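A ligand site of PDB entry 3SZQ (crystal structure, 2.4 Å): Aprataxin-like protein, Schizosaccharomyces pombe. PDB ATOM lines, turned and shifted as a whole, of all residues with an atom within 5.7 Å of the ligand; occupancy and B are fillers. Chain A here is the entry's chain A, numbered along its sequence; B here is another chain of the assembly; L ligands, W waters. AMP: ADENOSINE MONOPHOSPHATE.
The backbone NH of Met 38 lies within hydrogen-bond range of a nitrogen (N3) of the ligand, at 3.3 Å.
The side-chain carboxylate of Asp 37 sits at hydrogen-bond distance from an oxygen (O2') of the ligand (2.5 Å).
The backbone NH of Ser 116 is in hydrogen-bond range of an oxygen (O1P) of the ligand (2.7 Å).
ND1 of His 112 sits at hydrogen-bond distance from O3P of the ligand (3.0 Å).
An oxygen (O2P) of the ligand sits at hydrogen-bond distance from a ring nitrogen (NE2) of His 123.
N of Met 117 lies within hydrogen-bond range of O1P of the ligand (3.0 Å).
An oxygen (O2P) of the ligand sits at hydrogen-bond distance from a ring nitrogen (NE2) of His 121 (2.8 Å).
The side-chain amino group (NZ) of Lys 41 sits at hydrogen-bond distance from an oxygen (O2') of the ligand (3.3 Å).
The side-chain sulfur (SD) of Met 38 sits close to a nitrogen (N6) of the ligand (3.6 Å).
OH of Tyr 15 sits at hydrogen-bond distance from N1 of the ligand.
The side-chain amino group (NZ) of Lys 41 lies within salt-bridge range of OP1 of DC 2 of chain B, 2.8 Å away.
The backbone NH (N) of Leu 47 is in hydrogen-bond range of the backbone carbonyl oxygen (O) of Val 35 (2.8 Å).
The backbone NH (N) of Asp 37 is in hydrogen-bond range of the backbone carbonyl oxygen (O) of His 45 (2.9 Å).
The backbone carbonyl oxygen of Phe 39 sits at hydrogen-bond distance from the side-chain amino group of Lys 41 (2.9 Å).
OD1 of Asp 37 is in hydrogen-bond range of N of Phe 39 (2.9 Å).
A ring nitrogen (ND1) of His 123 lies within hydrogen-bond range of a ring nitrogen (NE2) of His 45.
N of Lys 41 is in hydrogen-bond range of ND1 of His 45 (2.8 Å).
Merely in contact with the ligand: Leu 12, Phe 39, His 45, Leu 47, Pro 115 and DC 1 of chain B.
Hydrophobic or aromatic side chains that line the ligand: Leu 12, Tyr 15, Met 38, Phe 39, His 45, Leu 47, His 112, Pro 115, Met 117, His 121 and His 123.
Within 4 Å of the ligand: Leu 12, Tyr 15, Asp 37, Met 38, Phe 39, Lys 41, His 45, Leu 47, His 112, Pro 115, Ser 116, Met 117, His 121, His 123 and DC 1 of chain B.
The nearest printed residue that does not touch the ligand is Arg 36 (4.02 Å).
Water W1 bridges an oxygen (O3') of the ligand (2.5 Å) and the side-chain amino group (NZ) of Lys 41 (2.8 Å).
Water W4 lies within hydrogen-bond range of an oxygen (O3P) of the ligand (2.6 Å), the backbone carbonyl oxygen (O) of Gly 114 (2.7 Å) and a ring nitrogen (ND1) of His 112 (3.5 Å).
Water W3 lies within hydrogen-bond range of an oxygen (O3P) of the ligand and a ring nitrogen (ND1) of His 112.
Water W5 lies within hydrogen-bond range of N6 of the ligand (3.1 Å) and ND2 of Asn 11 (3.4 Å).
Water W2 lies within hydrogen-bond range of the backbone NH (N) of His 112 (3.0 Å), the backbone carbonyl oxygen (O) of His 121 (3.1 Å) and an oxygen (O2P) of the ligand (3.2 Å).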
ATOM      1  N   ASN A  11     -16.301  -3.674  -7.396  1.00  0.00           N
ATOM      2  CA  ASN A  11     -15.806  -2.826  -8.472  1.00  0.00           C
ATOM      3  C   ASN A  11     -15.489  -3.498  -9.810  1.00  0.00           C
ATOM      4  O   ASN A  11     -15.594  -2.855 -10.854  1.00  0.00           O
ATOM      5  CB  ASN A  11     -14.591  -2.023  -7.990  1.00  0.00           C
ATOM      6  CG  ASN A  11     -14.980  -0.783  -7.205  1.00  0.00           C
ATOM      7  OD1 ASN A  11     -16.161  -0.521  -6.996  1.00  0.00           O
ATOM      8  ND2 ASN A  11     -13.994  -0.018  -6.773  1.00  0.00           N
ATOM      9  N   LEU A  12     -15.085  -4.768  -9.793  1.00  0.00           N
ATOM     10  CA  LEU A  12     -14.724  -5.461 -11.047  1.00  0.00           C
ATOM     11  C   LEU A  12     -15.964  -5.936 -11.805  1.00  0.00           C
ATOM     12  O   LEU A  12     -15.891  -6.335 -12.968  1.00  0.00           O
ATOM     13  CB  LEU A  12     -13.802  -6.649 -10.779  1.00  0.00           C
ATOM     14  CG  LEU A  12     -12.433  -6.373 -10.145  1.00  0.00           C
ATOM     15  CD1 LEU A  12     -11.563  -7.636 -10.158  1.00  0.00           C
ATOM     16  CD2 LEU A  12     -11.740  -5.203 -10.851  1.00  0.00           C
ATOM     17  N   TYR A  15     -17.118  -5.016 -15.472  1.00  0.00           N
ATOM     18  CA  TYR A  15     -16.392  -5.573 -16.609  1.00  0.00           C
ATOM     19  C   TYR A  15     -17.055  -6.813 -17.165  1.00  0.00           C
ATOM     20  O   TYR A  15     -16.993  -7.072 -18.361  1.00  0.00           O
ATOM     21  CB  TYR A  15     -14.941  -5.857 -16.239  1.00  0.00           C
ATOM     22  CG  TYR A  15     -14.192  -4.623 -15.822  1.00  0.00           C
ATOM     23  CD1 TYR A  15     -14.224  -3.475 -16.612  1.00  0.00           C
ATOM     24  CD2 TYR A  15     -13.482  -4.592 -14.629  1.00  0.00           C
ATOM     25  CE1 TYR A  15     -13.553  -2.336 -16.227  1.00  0.00           C
ATOM     26  CE2 TYR A  15     -12.819  -3.446 -14.235  1.00  0.00           C
ATOM     27  CZ  TYR A  15     -12.855  -2.318 -15.034  1.00  0.00           C
ATOM     28  OH  TYR A  15     -12.183  -1.194 -14.637  1.00  0.00           O
ATOM     29  N   VAL A  35      -9.327  -7.851 -19.051  1.00  0.00           N
ATOM     30  CA  VAL A  35      -9.329  -6.418 -18.825  1.00  0.00           C
ATOM     31  C   VAL A  35      -7.988  -6.009 -18.200  1.00  0.00           C
ATOM     32  O   VAL A  35      -7.398  -6.775 -17.444  1.00  0.00           O
ATOM     33  CB  VAL A  35     -10.513  -5.989 -17.918  1.00  0.00           C
ATOM     34  CG1 VAL A  35     -10.507  -6.772 -16.613  1.00  0.00           C
ATOM     35  CG2 VAL A  35     -10.477  -4.479 -17.647  1.00  0.00           C
ATOM     36  N   ARG A  36      -7.504  -4.823 -18.557  1.00  0.00           N
ATOM     37  CA  ARG A  36      -6.308  -4.260 -17.925  1.00  0.00           C
ATOM     38  C   ARG A  36      -6.530  -3.984 -16.446  1.00  0.00           C
ATOM     39  O   ARG A  36      -7.588  -3.490 -16.052  1.00  0.00           O
ATOM     40  CB  ARG A  36      -5.912  -2.954 -18.607  1.00  0.00           C
ATOM     41  CG  ARG A  36      -5.551  -3.099 -20.074  1.00  0.00           C
ATOM     42  CD  ARG A  36      -4.763  -1.896 -20.570  1.00  0.00           C
ATOM     43  NE  ARG A  36      -4.224  -2.162 -21.894  1.00  0.00           N
ATOM     44  CZ  ARG A  36      -4.807  -1.792 -23.029  1.00  0.00           C
ATOM     45  NH1 ARG A  36      -5.956  -1.132 -22.997  1.00  0.00           N
ATOM     46  NH2 ARG A  36      -4.241  -2.083 -24.194  1.00  0.00           N
ATOM     47  N   ASP A  37      -5.538  -4.292 -15.623  1.00  0.00           N
ATOM     48  CA  ASP A  37      -5.578  -3.949 -14.198  1.00  0.00           C
ATOM     49  C   ASP A  37      -5.416  -2.443 -14.065  1.00  0.00           C
ATOM     50  O   ASP A  37      -4.469  -1.858 -14.600  1.00  0.00           O
ATOM     51  CB  ASP A  37      -4.467  -4.655 -13.426  1.00  0.00           C
ATOM     52  CG  ASP A  37      -4.717  -4.671 -11.924  1.00  0.00           C
ATOM     53  OD1 ASP A  37      -4.607  -3.598 -11.274  1.00  0.00           O
ATOM     54  OD2 ASP A  37      -5.024  -5.760 -11.392  1.00  0.00           O
ATOM     55  N   MET A  38      -6.334  -1.803 -13.340  1.00  0.00           N
ATOM     56  CA  MET A  38      -6.327  -0.353 -13.237  1.00  0.00           C
ATOM     57  C   MET A  38      -5.134   0.151 -12.423  1.00  0.00           C
ATOM     58  O   MET A  38      -4.739   1.313 -12.536  1.00  0.00           O
ATOM     59  CB  MET A  38      -7.642   0.134 -12.632  1.00  0.00           C
ATOM     60  CG  MET A  38      -7.681   1.625 -12.364  1.00  0.00           C
ATOM     61  SD  MET A  38      -9.304   2.123 -11.761  1.00  0.00           S
ATOM     62  CE  MET A  38     -10.301   1.685 -13.202  1.00  0.00           C
ATOM     63  N   PHE A  39      -4.565  -0.733 -11.604  1.00  0.00           N
ATOM     64  CA  PHE A  39      -3.418  -0.396 -10.772  1.00  0.00           C
ATOM     65  C   PHE A  39      -2.319  -1.445 -10.946  1.00  0.00           C
ATOM     66  O   PHE A  39      -1.964  -2.139 -10.010  1.00  0.00           O
ATOM     67  CB  PHE A  39      -3.837  -0.324  -9.295  1.00  0.00           C
ATOM     68  CG  PHE A  39      -4.985   0.609  -9.038  1.00  0.00           C
ATOM     69  CD1 PHE A  39      -4.772   1.963  -8.874  1.00  0.00           C
ATOM     70  CD2 PHE A  39      -6.287   0.127  -8.978  1.00  0.00           C
ATOM     71  CE1 PHE A  39      -5.831   2.815  -8.642  1.00  0.00           C
ATOM     72  CE2 PHE A  39      -7.355   0.973  -8.738  1.00  0.00           C
ATOM     73  CZ  PHE A  39      -7.121   2.330  -8.569  1.00  0.00           C
ATOM     74  N   PRO A  40      -1.762  -1.536 -12.167  1.00  0.00           N
ATOM     75  CA  PRO A  40      -0.861  -2.634 -12.550  1.00  0.00           C
ATOM     76  C   PRO A  40       0.306  -2.798 -11.590  1.00  0.00           C
ATOM     77  O   PRO A  40       0.955  -1.818 -11.227  1.00  0.00           O
ATOM     78  CB  PRO A  40      -0.374  -2.220 -13.955  1.00  0.00           C
ATOM     79  CG  PRO A  40      -0.609  -0.724 -14.021  1.00  0.00           C
ATOM     80  CD  PRO A  40      -1.841  -0.488 -13.206  1.00  0.00           C
ATOM     81  N   LYS A  41       0.575  -4.022 -11.175  1.00  0.00           N
ATOM     82  CA  LYS A  41       1.670  -4.246 -10.238  1.00  0.00           C
ATOM     83  C   LYS A  41       2.946  -4.703 -10.962  1.00  0.00           C
ATOM     84  O   LYS A  41       3.976  -4.947 -10.348  1.00  0.00           O
ATOM     85  CB  LYS A  41       1.260  -5.208  -9.132  1.00  0.00           C
ATOM     86  CG  LYS A  41       0.031  -4.728  -8.334  1.00  0.00           C
ATOM     87  CD  LYS A  41       0.244  -3.318  -7.765  1.00  0.00           C
ATOM     88  CE  LYS A  41      -0.831  -2.927  -6.751  1.00  0.00           C
ATOM     89  NZ  LYS A  41      -2.225  -3.020  -7.303  1.00  0.00           N
ATOM     90  N   HIS A  45      -0.098  -6.031 -16.635  1.00  0.00           N
ATOM     91  CA  HIS A  45      -0.932  -6.632 -15.601  1.00  0.00           C
ATOM     92  C   HIS A  45      -2.378  -6.668 -16.079  1.00  0.00           C
ATOM     93  O   HIS A  45      -3.031  -5.622 -16.200  1.00  0.00           O
ATOM     94  CB  HIS A  45      -0.789  -5.860 -14.275  1.00  0.00           C
ATOM     95  CG  HIS A  45      -1.391  -6.561 -13.092  1.00  0.00           C
ATOM     96  ND1 HIS A  45      -1.249  -6.101 -11.801  1.00  0.00           N
ATOM     97  CD2 HIS A  45      -2.146  -7.696 -13.006  1.00  0.00           C
ATOM     98  CE1 HIS A  45      -1.879  -6.910 -10.971  1.00  0.00           C
ATOM     99  NE2 HIS A  45      -2.429  -7.892 -11.678  1.00  0.00           N
ATOM    100  N   LEU A  47      -6.324  -8.918 -16.075  1.00  0.00           N
ATOM    101  CA  LEU A  47      -7.191  -9.779 -15.281  1.00  0.00           C
ATOM    102  C   LEU A  47      -8.109 -10.551 -16.217  1.00  0.00           C
ATOM    103  O   LEU A  47      -8.784  -9.953 -17.049  1.00  0.00           O
ATOM    104  CB  LEU A  47      -8.048  -8.949 -14.293  1.00  0.00           C
ATOM    105  CG  LEU A  47      -7.334  -7.948 -13.382  1.00  0.00           C
ATOM    106  CD1 LEU A  47      -8.329  -7.111 -12.585  1.00  0.00           C
ATOM    107  CD2 LEU A  47      -6.332  -8.647 -12.438  1.00  0.00           C
ATOM    108  N   HIS A 112      -4.868 -14.709  -6.376  1.00  0.00           N
ATOM    109  CA  HIS A 112      -4.521 -14.405  -4.987  1.00  0.00           C
ATOM    110  C   HIS A 112      -5.288 -15.334  -4.060  1.00  0.00           C
ATOM    111  O   HIS A 112      -6.484 -15.558  -4.242  1.00  0.00           O
ATOM    112  CB  HIS A 112      -4.878 -12.966  -4.640  1.00  0.00           C
ATOM    113  CG  HIS A 112      -3.780 -11.994  -4.927  1.00  0.00           C
ATOM    114  ND1 HIS A 112      -3.975 -10.631  -4.921  1.00  0.00           N
ATOM    115  CD2 HIS A 112      -2.471 -12.187  -5.202  1.00  0.00           C
ATOM    116  CE1 HIS A 112      -2.833 -10.023  -5.199  1.00  0.00           C
ATOM    117  NE2 HIS A 112      -1.905 -10.949  -5.373  1.00  0.00           N
ATOM    118  N   GLY A 114      -6.147 -14.795  -1.016  1.00  0.00           N
ATOM    119  CA  GLY A 114      -7.176 -14.005  -0.370  1.00  0.00           C
ATOM    120  C   GLY A 114      -7.458 -12.732  -1.153  1.00  0.00           C
ATOM    121  O   GLY A 114      -6.803 -11.719  -0.938  1.00  0.00           O
ATOM    122  N   PRO A 115      -8.444 -12.775  -2.060  1.00  0.00           N
ATOM    123  CA  PRO A 115      -8.773 -11.633  -2.907  1.00  0.00           C
ATOM    124  C   PRO A 115      -9.396 -10.502  -2.099  1.00  0.00           C
ATOM    125  O   PRO A 115      -9.977 -10.778  -1.059  1.00  0.00           O
ATOM    126  CB  PRO A 115      -9.835 -12.184  -3.864  1.00  0.00           C
ATOM    127  CG  PRO A 115      -9.884 -13.651  -3.637  1.00  0.00           C
ATOM    128  CD  PRO A 115      -9.376 -13.896  -2.266  1.00  0.00           C
ATOM    129  N   SER A 116      -9.275  -9.258  -2.574  1.00  0.00           N
ATOM    130  CA  SER A 116     -10.050  -8.156  -2.017  1.00  0.00           C
ATOM    131  C   SER A 116     -11.308  -7.928  -2.846  1.00  0.00           C
ATOM    132  O   SER A 116     -12.358  -7.612  -2.307  1.00  0.00           O
ATOM    133  CB  SER A 116      -9.242  -6.869  -1.965  1.00  0.00           C
ATOM    134  OG  SER A 116      -8.107  -7.010  -1.134  1.00  0.00           O
ATOM    135  N   MET A 117     -11.188  -8.112  -4.159  1.00  0.00           N
ATOM    136  CA  MET A 117     -12.355  -7.991  -5.044  1.00  0.00           C
ATOM    137  C   MET A 117     -13.111  -9.303  -5.130  1.00  0.00           C
ATOM    138  O   MET A 117     -12.510 -10.372  -5.161  1.00  0.00           O
ATOM    139  CB  MET A 117     -11.924  -7.535  -6.442  1.00  0.00           C
ATOM    140  CG  MET A 117     -11.166  -6.243  -6.446  1.00  0.00           C
ATOM    141  SD  MET A 117     -12.208  -4.823  -6.023  1.00  0.00           S
ATOM    142  CE  MET A 117     -10.946  -3.566  -5.888  1.00  0.00           C
ATOM    143  N   HIS A 121     -11.098 -13.402 -10.525  1.00  0.00           N
ATOM    144  CA  HIS A 121     -10.236 -12.834 -11.553  1.00  0.00           C
ATOM    145  C   HIS A 121      -8.848 -13.463 -11.478  1.00  0.00           C
ATOM    146  O   HIS A 121      -8.248 -13.572 -10.405  1.00  0.00           O
ATOM    147  CB  HIS A 121     -10.123 -11.320 -11.360  1.00  0.00           C
ATOM    148  CG  HIS A 121      -9.743 -10.913  -9.973  1.00  0.00           C
ATOM    149  ND1 HIS A 121     -10.641 -10.905  -8.932  1.00  0.00           N
ATOM    150  CD2 HIS A 121      -8.550 -10.547  -9.456  1.00  0.00           C
ATOM    151  CE1 HIS A 121     -10.021 -10.525  -7.828  1.00  0.00           C
ATOM    152  NE2 HIS A 121      -8.751 -10.305  -8.115  1.00  0.00           N
ATOM    153  N   HIS A 123      -4.971 -13.220 -12.396  1.00  0.00           N
ATOM    154  CA  HIS A 123      -3.894 -12.302 -12.765  1.00  0.00           C
ATOM    155  C   HIS A 123      -2.963 -12.900 -13.820  1.00  0.00           C
ATOM    156  O   HIS A 123      -2.504 -14.036 -13.704  1.00  0.00           O
ATOM    157  CB  HIS A 123      -3.050 -11.947 -11.545  1.00  0.00           C
ATOM    158  CG  HIS A 123      -3.825 -11.347 -10.417  1.00  0.00           C
ATOM    159  ND1 HIS A 123      -3.971  -9.990 -10.260  1.00  0.00           N
ATOM    160  CD2 HIS A 123      -4.458 -11.925  -9.365  1.00  0.00           C
ATOM    161  CE1 HIS A 123      -4.681  -9.753  -9.169  1.00  0.00           C
ATOM    162  NE2 HIS A 123      -4.980 -10.909  -8.610  1.00  0.00           N
ATOM    163  N   PHE A 143       2.325 -11.174  -4.693  1.00  0.00           N
ATOM    164  CA  PHE A 143       2.532 -11.732  -6.028  1.00  0.00           C
ATOM    165  C   PHE A 143       3.772 -12.610  -6.157  1.00  0.00           C
ATOM    166  O   PHE A 143       3.997 -13.210  -7.210  1.00  0.00           O
ATOM    167  CB  PHE A 143       2.568 -10.611  -7.093  1.00  0.00           C
ATOM    168  CG  PHE A 143       1.235  -9.994  -7.359  1.00  0.00           C
ATOM    169  CD1 PHE A 143       0.280 -10.663  -8.118  1.00  0.00           C
ATOM    170  CD2 PHE A 143       0.917  -8.738  -6.859  1.00  0.00           C
ATOM    171  CE1 PHE A 143      -0.963 -10.094  -8.369  1.00  0.00           C
ATOM    172  CE2 PHE A 143      -0.322  -8.165  -7.089  1.00  0.00           C
ATOM    173  CZ  PHE A 143      -1.259  -8.850  -7.852  1.00  0.00           C
ATOM    174  O5'  DC B   1      -5.639  -4.764  -2.510  1.00  0.00           O
ATOM    175  C5'  DC B   1      -6.498  -5.130  -3.584  1.00  0.00           C
ATOM    176  C4'  DC B   1      -7.145  -3.911  -4.207  1.00  0.00           C
ATOM    177  O4'  DC B   1      -8.494  -3.810  -3.712  1.00  0.00           O
ATOM    178  C3'  DC B   1      -6.503  -2.547  -3.893  1.00  0.00           C
ATOM    179  O3'  DC B   1      -5.509  -2.225  -4.835  1.00  0.00           O
ATOM    180  C2'  DC B   1      -7.696  -1.600  -4.046  1.00  0.00           C
ATOM    181  C1'  DC B   1      -8.833  -2.456  -3.486  1.00  0.00           C
ATOM    182  N1   DC B   1      -9.088  -2.252  -2.031  1.00  0.00           N
ATOM    183  C2   DC B   1      -9.853  -1.144  -1.642  1.00  0.00           C
ATOM    184  O2   DC B   1     -10.270  -0.368  -2.522  1.00  0.00           O
ATOM    185  N3   DC B   1     -10.094  -0.959  -0.322  1.00  0.00           N
ATOM    186  C4   DC B   1      -9.621  -1.830   0.581  1.00  0.00           C
ATOM    187  N4   DC B   1      -9.896  -1.602   1.861  1.00  0.00           N
ATOM    188  C5   DC B   1      -8.848  -2.969   0.201  1.00  0.00           C
ATOM    189  C6   DC B   1      -8.602  -3.134  -1.111  1.00  0.00           C
ATOM    190  P    DC B   2      -4.321  -1.209  -4.454  1.00  0.00           P
ATOM    191  OP1  DC B   2      -3.394  -1.140  -5.607  1.00  0.00           O
ATOM    192  OP2  DC B   2      -3.798  -1.609  -3.132  1.00  0.00           O
ATOM    193  O5'  DC B   2      -5.069   0.191  -4.310  1.00  0.00           O
ATOM    194  C5'  DC B   2      -5.706   0.835  -5.404  1.00  0.00           C
ATOM    195  C4'  DC B   2      -6.326   2.122  -4.897  1.00  0.00           C
ATOM    196  O4'  DC B   2      -7.282   1.738  -3.876  1.00  0.00           O
ATOM    197  C3'  DC B   2      -5.327   3.050  -4.219  1.00  0.00           C
ATOM    198  O3'  DC B   2      -5.009   4.203  -5.005  1.00  0.00           O
ATOM    199  C2'  DC B   2      -5.995   3.484  -2.918  1.00  0.00           C
ATOM    200  C1'  DC B   2      -7.287   2.692  -2.843  1.00  0.00           C
ATOM    201  N1   DC B   2      -7.406   2.037  -1.516  1.00  0.00           N
ATOM    202  C2   DC B   2      -8.199   2.692  -0.573  1.00  0.00           C
ATOM    203  O2   DC B   2      -8.754   3.733  -0.929  1.00  0.00           O
ATOM    204  N3   DC B   2      -8.352   2.157   0.666  1.00  0.00           N
ATOM    205  C4   DC B   2      -7.734   1.019   0.978  1.00  0.00           C
ATOM    206  N4   DC B   2      -7.913   0.531   2.212  1.00  0.00           N
ATOM    207  C5   DC B   2      -6.903   0.346   0.027  1.00  0.00           C
ATOM    208  C6   DC B   2      -6.768   0.882  -1.194  1.00  0.00           C
HETATM  209  P   AMP L   1      -7.101  -9.204  -5.509  1.00  0.00           P
HETATM  210  O1P AMP L   1      -8.552  -8.966  -5.204  1.00  0.00           O
HETATM  211  O2P AMP L   1      -6.787 -10.567  -6.078  1.00  0.00           O
HETATM  212  O3P AMP L   1      -6.152  -8.688  -4.477  1.00  0.00           O
HETATM  213  O5' AMP L   1      -6.732  -8.288  -6.750  1.00  0.00           O
HETATM  214  C5' AMP L   1      -7.618  -7.274  -7.217  1.00  0.00           C
HETATM  215  C4' AMP L   1      -7.002  -6.522  -8.354  1.00  0.00           C
HETATM  216  O4' AMP L   1      -7.973  -5.615  -8.933  1.00  0.00           O
HETATM  217  C3' AMP L   1      -5.782  -5.674  -7.976  1.00  0.00           C
HETATM  218  O3' AMP L   1      -4.679  -6.050  -8.798  1.00  0.00           O
HETATM  219  C2' AMP L   1      -6.215  -4.222  -8.308  1.00  0.00           C
HETATM  220  O2' AMP L   1      -5.176  -3.408  -8.819  1.00  0.00           O
HETATM  221  C1' AMP L   1      -7.323  -4.439  -9.328  1.00  0.00           C
HETATM  222  N9  AMP L   1      -8.339  -3.382  -9.370  1.00  0.00           N
HETATM  223  C8  AMP L   1      -8.867  -2.750  -8.310  1.00  0.00           C
HETATM  224  N7  AMP L   1      -9.829  -1.890  -8.708  1.00  0.00           N
HETATM  225  C5  AMP L   1      -9.927  -1.973 -10.044  1.00  0.00           C
HETATM  226  C6  AMP L   1     -10.751  -1.329 -11.098  1.00  0.00           C
HETATM  227  N6  AMP L   1     -11.671  -0.388 -10.779  1.00  0.00           N
HETATM  228  N1  AMP L   1     -10.554  -1.705 -12.381  1.00  0.00           N
HETATM  229  C2  AMP L   1      -9.632  -2.632 -12.698  1.00  0.00           C
HETATM  230  N3  AMP L   1      -8.853  -3.243 -11.792  1.00  0.00           N
HETATM  231  C4  AMP L   1      -8.951  -2.962 -10.472  1.00  0.00           C
HETATM  232  O   HOH W   1      -2.877  -5.702  -7.113  1.00  0.00           O
HETATM  233  O   HOH W   2      -7.360 -13.367  -7.403  1.00  0.00           O
HETATM  234  O   HOH W   3      -3.962  -7.133  -4.914  1.00  0.00           O
HETATM  235  O   HOH W   4      -5.660  -9.560  -2.068  1.00  0.00           O
HETATM  236  O   HOH W   5     -11.698   1.813  -8.541  1.00  0.00           O
